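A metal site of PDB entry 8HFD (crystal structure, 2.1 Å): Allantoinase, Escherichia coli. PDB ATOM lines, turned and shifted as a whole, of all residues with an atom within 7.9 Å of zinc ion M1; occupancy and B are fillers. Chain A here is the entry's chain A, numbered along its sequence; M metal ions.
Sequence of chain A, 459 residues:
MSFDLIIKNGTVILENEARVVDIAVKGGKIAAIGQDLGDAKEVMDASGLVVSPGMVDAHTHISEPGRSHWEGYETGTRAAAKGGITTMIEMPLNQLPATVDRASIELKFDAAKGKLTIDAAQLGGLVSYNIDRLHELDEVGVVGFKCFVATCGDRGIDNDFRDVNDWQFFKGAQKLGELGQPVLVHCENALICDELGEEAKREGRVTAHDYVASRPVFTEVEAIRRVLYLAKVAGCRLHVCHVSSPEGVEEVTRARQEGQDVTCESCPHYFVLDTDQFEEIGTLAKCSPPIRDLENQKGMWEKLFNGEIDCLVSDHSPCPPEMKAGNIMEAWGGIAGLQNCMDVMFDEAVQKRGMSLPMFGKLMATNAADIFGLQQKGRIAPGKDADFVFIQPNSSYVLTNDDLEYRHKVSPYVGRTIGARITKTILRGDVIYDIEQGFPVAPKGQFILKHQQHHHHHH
Zinc ion M1 is bound by OQ2 of KCX 146. Zinc ion M1 is bound by ND1 of His 186. Zinc ion M1 is bound by a ring nitrogen (NE2) of His 242 (2.2 Å).
Merely in contact with zinc ion M1: Phe 148 (3.99 Å). Within 4 Å of zinc ion M1: KCX 146, Phe 148, His 186 and His 242. The nearest printed residue that does not touch zinc ion M1 is His 59 (4.1 Å).
N of His 186 is in hydrogen-bond range of O of Cys 147 (3.1 Å). The side-chain hydroxyl (OG) of Ser 288 is in hydrogen-bond range of a ring nitrogen (NE2) of His 186 (3.1 Å). N of His 242 is in hydrogen-bond range of OE2 of Glu 265 (2.9 Å). The side-chain sulfur of Met 91 lies close to NZ of KCX 146 (3.4 Å). NE2 of His 61 sits close to OQ1 of KCX 146 (3.3 Å). A ring nitrogen (NE2) of His 186 sits at hydrogen-bond distance from the side-chain carboxylate (OE1) of Glu 188, 2.9 Å away.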
ATOM      1  N   HIS A  59      27.686  -1.924  16.422  1.00  0.00           N
ATOM      2  CA  HIS A  59      28.213  -1.304  15.216  1.00  0.00           C
ATOM      3  C   HIS A  59      28.232   0.212  15.343  1.00  0.00           C
ATOM      4  O   HIS A  59      27.330   0.900  14.845  1.00  0.00           O
ATOM      5  CB  HIS A  59      27.363  -1.767  14.021  1.00  0.00           C
ATOM      6  CG  HIS A  59      28.012  -1.536  12.694  1.00  0.00           C
ATOM      7  ND1 HIS A  59      27.938  -2.453  11.674  1.00  0.00           N
ATOM      8  CD2 HIS A  59      28.722  -0.484  12.220  1.00  0.00           C
ATOM      9  CE1 HIS A  59      28.570  -1.969  10.611  1.00  0.00           C
ATOM     10  NE2 HIS A  59      29.047  -0.784  10.921  1.00  0.00           N
ATOM     11  N   HIS A  61      30.518   3.822  14.969  1.00  0.00           N
ATOM     12  CA  HIS A  61      31.687   4.599  14.547  1.00  0.00           C
ATOM     13  C   HIS A  61      31.822   5.833  15.419  1.00  0.00           C
ATOM     14  O   HIS A  61      30.944   6.704  15.393  1.00  0.00           O
ATOM     15  CB  HIS A  61      31.585   5.015  13.081  1.00  0.00           C
ATOM     16  CG  HIS A  61      31.568   3.854  12.140  1.00  0.00           C
ATOM     17  ND1 HIS A  61      32.701   3.122  11.851  1.00  0.00           N
ATOM     18  CD2 HIS A  61      30.560   3.292  11.436  1.00  0.00           C
ATOM     19  CE1 HIS A  61      32.390   2.161  11.017  1.00  0.00           C
ATOM     20  NE2 HIS A  61      31.101   2.241  10.746  1.00  0.00           N
ATOM     21  N   MET A  91      33.779   0.116  16.148  1.00  0.00           N
ATOM     22  CA  MET A  91      34.448  -0.241  14.880  1.00  0.00           C
ATOM     23  C   MET A  91      35.881   0.319  14.846  1.00  0.00           C
ATOM     24  O   MET A  91      36.129   1.313  15.520  1.00  0.00           O
ATOM     25  CB  MET A  91      33.633   0.352  13.729  1.00  0.00           C
ATOM     26  CG  MET A  91      32.372  -0.430  13.426  1.00  0.00           C
ATOM     27  SD  MET A  91      32.769  -2.047  12.735  1.00  0.00           S
ATOM     28  CE  MET A  91      31.204  -2.897  12.971  1.00  0.00           C
ATOM     29  N   LEU A  93      37.264   1.937  12.535  1.00  0.00           N
ATOM     30  CA  LEU A  93      37.280   3.143  11.679  1.00  0.00           C
ATOM     31  C   LEU A  93      36.118   4.051  12.114  1.00  0.00           C
ATOM     32  O   LEU A  93      35.180   3.530  12.681  1.00  0.00           O
ATOM     33  CB  LEU A  93      37.136   2.707  10.216  1.00  0.00           C
ATOM     34  CG  LEU A  93      35.767   2.172   9.803  1.00  0.00           C
ATOM     35  CD1 LEU A  93      35.607   2.225   8.287  1.00  0.00           C
ATOM     36  CD2 LEU A  93      35.553   0.757  10.296  1.00  0.00           C
ATOM     37  N   KCX A 146      36.832  -6.335  11.826  1.00  0.00           N
ATOM     38  CA  KCX A 146      35.910  -5.849  10.767  1.00  0.00           C
ATOM     39  CB  KCX A 146      35.143  -4.610  11.234  1.00  0.00           C
ATOM     40  CG  KCX A 146      33.663  -4.598  10.869  1.00  0.00           C
ATOM     41  CD  KCX A 146      33.384  -4.632   9.386  1.00  0.00           C
ATOM     42  CE  KCX A 146      33.239  -3.259   8.758  1.00  0.00           C
ATOM     43  NZ  KCX A 146      32.176  -2.480   9.365  1.00  0.00           N
ATOM     44  C   KCX A 146      36.670  -5.554   9.477  1.00  0.00           C
ATOM     45  O   KCX A 146      37.768  -4.964   9.557  1.00  0.00           O
ATOM     46  CX  KCX A 146      31.594  -1.448   8.721  1.00  0.00           C
ATOM     47  OQ1 KCX A 146      31.940  -0.301   8.866  1.00  0.00           O
ATOM     48  OQ2 KCX A 146      30.617  -1.814   7.907  1.00  0.00           O
ATOM     49  N   CYS A 147      36.119  -5.968   8.339  1.00  0.00           N
ATOM     50  CA  CYS A 147      36.714  -5.691   7.041  1.00  0.00           C
ATOM     51  C   CYS A 147      35.701  -5.349   5.950  1.00  0.00           C
ATOM     52  O   CYS A 147      34.487  -5.589   6.099  1.00  0.00           O
ATOM     53  CB  CYS A 147      37.557  -6.883   6.598  1.00  0.00           C
ATOM     54  SG  CYS A 147      36.591  -8.313   6.088  1.00  0.00           S
ATOM     55  N   PHE A 148      36.216  -4.730   4.881  1.00  0.00           N
ATOM     56  CA  PHE A 148      35.496  -4.494   3.635  1.00  0.00           C
ATOM     57  C   PHE A 148      36.195  -5.301   2.550  1.00  0.00           C
ATOM     58  O   PHE A 148      37.395  -5.152   2.350  1.00  0.00           O
ATOM     59  CB  PHE A 148      35.517  -3.019   3.224  1.00  0.00           C
ATOM     60  CG  PHE A 148      34.684  -2.111   4.064  1.00  0.00           C
ATOM     61  CD1 PHE A 148      34.944  -1.941   5.411  1.00  0.00           C
ATOM     62  CD2 PHE A 148      33.661  -1.371   3.485  1.00  0.00           C
ATOM     63  CE1 PHE A 148      34.183  -1.064   6.179  1.00  0.00           C
ATOM     64  CE2 PHE A 148      32.891  -0.498   4.253  1.00  0.00           C
ATOM     65  CZ  PHE A 148      33.161  -0.355   5.609  1.00  0.00           C
ATOM     66  N   VAL A 185      31.821  -8.209   8.237  1.00  0.00           N
ATOM     67  CA  VAL A 185      32.055  -7.733   6.854  1.00  0.00           C
ATOM     68  C   VAL A 185      30.961  -6.797   6.334  1.00  0.00           C
ATOM     69  O   VAL A 185      29.797  -7.092   6.530  1.00  0.00           O
ATOM     70  CB  VAL A 185      32.223  -8.922   5.894  1.00  0.00           C
ATOM     71  CG1 VAL A 185      32.600  -8.478   4.496  1.00  0.00           C
ATOM     72  CG2 VAL A 185      33.199  -9.968   6.410  1.00  0.00           C
ATOM     73  N   HIS A 186      31.380  -5.685   5.722  1.00  0.00           N
ATOM     74  CA  HIS A 186      30.437  -4.812   4.997  1.00  0.00           C
ATOM     75  C   HIS A 186      30.299  -5.481   3.631  1.00  0.00           C
ATOM     76  O   HIS A 186      31.267  -5.460   2.880  1.00  0.00           O
ATOM     77  CB  HIS A 186      30.954  -3.369   4.947  1.00  0.00           C
ATOM     78  CG  HIS A 186      30.145  -2.432   4.136  1.00  0.00           C
ATOM     79  ND1 HIS A 186      29.618  -1.272   4.673  1.00  0.00           N
ATOM     80  CD2 HIS A 186      29.796  -2.440   2.832  1.00  0.00           C
ATOM     81  CE1 HIS A 186      28.957  -0.627   3.739  1.00  0.00           C
ATOM     82  NE2 HIS A 186      29.054  -1.320   2.607  1.00  0.00           N
ATOM     83  N   CYS A 187      29.131  -6.070   3.368  1.00  0.00           N
ATOM     84  CA  CYS A 187      28.941  -6.893   2.161  1.00  0.00           C
ATOM     85  C   CYS A 187      28.224  -6.143   1.040  1.00  0.00           C
ATOM     86  O   CYS A 187      26.997  -6.216   0.971  1.00  0.00           O
ATOM     87  CB  CYS A 187      28.210  -8.173   2.546  1.00  0.00           C
ATOM     88  SG  CYS A 187      29.115  -9.241   3.687  1.00  0.00           S
ATOM     89  N   GLU A 188      28.985  -5.486   0.178  1.00  0.00           N
ATOM     90  CA  GLU A 188      28.423  -4.814  -1.007  1.00  0.00           C
ATOM     91  C   GLU A 188      29.475  -4.953  -2.110  1.00  0.00           C
ATOM     92  O   GLU A 188      30.648  -4.772  -1.807  1.00  0.00           O
ATOM     93  CB  GLU A 188      28.175  -3.336  -0.745  1.00  0.00           C
ATOM     94  CG  GLU A 188      26.780  -2.942  -0.289  1.00  0.00           C
ATOM     95  CD  GLU A 188      26.631  -1.427  -0.312  1.00  0.00           C
ATOM     96  OE1 GLU A 188      27.506  -0.740   0.245  1.00  0.00           O
ATOM     97  OE2 GLU A 188      25.667  -0.943  -0.914  1.00  0.00           O
ATOM     98  N   CYS A 241      27.314  -7.614   8.402  1.00  0.00           N
ATOM     99  CA  CYS A 241      26.936  -6.311   8.940  1.00  0.00           C
ATOM    100  C   CYS A 241      25.731  -5.758   8.207  1.00  0.00           C
ATOM    101  O   CYS A 241      25.475  -6.094   7.054  1.00  0.00           O
ATOM    102  CB  CYS A 241      28.111  -5.323   8.831  1.00  0.00           C
ATOM    103  SG  CYS A 241      29.454  -5.668   9.989  1.00  0.00           S
ATOM    104  N   HIS A 242      25.010  -4.852   8.891  1.00  0.00           N
ATOM    105  CA  HIS A 242      23.823  -4.154   8.397  1.00  0.00           C
ATOM    106  C   HIS A 242      23.239  -4.692   7.096  1.00  0.00           C
ATOM    107  O   HIS A 242      23.498  -4.133   6.023  1.00  0.00           O
ATOM    108  CB  HIS A 242      24.158  -2.676   8.185  1.00  0.00           C
ATOM    109  CG  HIS A 242      25.460  -2.474   7.483  1.00  0.00           C
ATOM    110  ND1 HIS A 242      25.814  -3.192   6.368  1.00  0.00           N
ATOM    111  CD2 HIS A 242      26.503  -1.655   7.764  1.00  0.00           C
ATOM    112  CE1 HIS A 242      27.021  -2.825   5.982  1.00  0.00           C
ATOM    113  NE2 HIS A 242      27.464  -1.898   6.809  1.00  0.00           N
ATOM    114  N   GLU A 265      23.049  -8.786  11.183  1.00  0.00           N
ATOM    115  CA  GLU A 265      22.459  -7.673  11.910  1.00  0.00           C
ATOM    116  C   GLU A 265      21.765  -6.788  10.893  1.00  0.00           C
ATOM    117  O   GLU A 265      21.988  -6.929   9.677  1.00  0.00           O
ATOM    118  CB  GLU A 265      23.528  -6.873  12.687  1.00  0.00           C
ATOM    119  CG  GLU A 265      24.209  -5.837  11.779  1.00  0.00           C
ATOM    120  CD  GLU A 265      25.573  -5.334  12.264  1.00  0.00           C
ATOM    121  OE1 GLU A 265      26.054  -5.722  13.355  1.00  0.00           O
ATOM    122  OE2 GLU A 265      26.157  -4.500  11.518  1.00  0.00           O
ATOM    123  N   TYR A 270      16.712   0.751   8.185  1.00  0.00           N
ATOM    124  CA  TYR A 270      16.171  -0.160   7.185  1.00  0.00           C
ATOM    125  C   TYR A 270      14.791  -0.686   7.548  1.00  0.00           C
ATOM    126  O   TYR A 270      14.172  -1.356   6.710  1.00  0.00           O
ATOM    127  CB  TYR A 270      17.138  -1.335   6.953  1.00  0.00           C
ATOM    128  CG  TYR A 270      18.528  -0.906   6.555  1.00  0.00           C
ATOM    129  CD1 TYR A 270      18.740  -0.202   5.369  1.00  0.00           C
ATOM    130  CD2 TYR A 270      19.618  -1.159   7.372  1.00  0.00           C
ATOM    131  CE1 TYR A 270      19.987   0.198   5.003  1.00  0.00           C
ATOM    132  CE2 TYR A 270      20.883  -0.752   7.008  1.00  0.00           C
ATOM    133  CZ  TYR A 270      21.065  -0.080   5.824  1.00  0.00           C
ATOM    134  OH  TYR A 270      22.333   0.328   5.429  1.00  0.00           O
ATOM    135  N   SER A 288      25.387   3.595   2.885  1.00  0.00           N
ATOM    136  CA  SER A 288      26.062   2.679   1.931  1.00  0.00           C
ATOM    137  C   SER A 288      25.141   1.535   1.585  1.00  0.00           C
ATOM    138  O   SER A 288      24.655   1.561   0.455  1.00  0.00           O
ATOM    139  CB  SER A 288      27.422   2.209   2.387  1.00  0.00           C
ATOM    140  OG  SER A 288      28.045   1.402   1.413  1.00  0.00           O
ATOM    141  N   PRO A 289      24.859   0.537   2.446  1.00  0.00           N
ATOM    142  CA  PRO A 289      23.855  -0.419   2.085  1.00  0.00           C
ATOM    143  C   PRO A 289      22.694   0.596   2.058  1.00  0.00           C
ATOM    144  O   PRO A 289      22.448   1.238   3.036  1.00  0.00           O
ATOM    145  CB  PRO A 289      23.836  -1.465   3.213  1.00  0.00           C
ATOM    146  CG  PRO A 289      25.028  -1.107   4.073  1.00  0.00           C
ATOM    147  CD  PRO A 289      25.385   0.332   3.792  1.00  0.00           C
ATOM    148  N   ASP A 315      24.897   1.407  13.255  1.00  0.00           N
ATOM    149  CA  ASP A 315      25.810   1.886  12.208  1.00  0.00           C
ATOM    150  C   ASP A 315      25.915   3.398  12.236  1.00  0.00           C
ATOM    151  O   ASP A 315      25.867   4.071  11.197  1.00  0.00           O
ATOM    152  CB  ASP A 315      25.408   1.402  10.813  1.00  0.00           C
ATOM    153  CG  ASP A 315      26.515   1.656   9.783  1.00  0.00           C
ATOM    154  OD1 ASP A 315      27.657   1.999  10.203  1.00  0.00           O
ATOM    155  OD2 ASP A 315      26.254   1.511   8.576  1.00  0.00           O
ATOM    156  N   SER A 317      27.038   6.695  11.778  1.00  0.00           N
ATOM    157  CA  SER A 317      27.991   7.094  10.751  1.00  0.00           C
ATOM    158  C   SER A 317      27.898   8.598  10.510  1.00  0.00           C
ATOM    159  O   SER A 317      27.499   9.045   9.440  1.00  0.00           O
ATOM    160  CB  SER A 317      27.737   6.319   9.455  1.00  0.00           C
ATOM    161  OG  SER A 317      27.991   4.940   9.632  1.00  0.00           O
HETATM  162 ZN    ZN M   1      29.362  -0.782   6.737  1.00  0.00          ZN
HETATM  163 ZN    ZN M   2      29.682   0.925   9.649  1.00  0.00          ZN
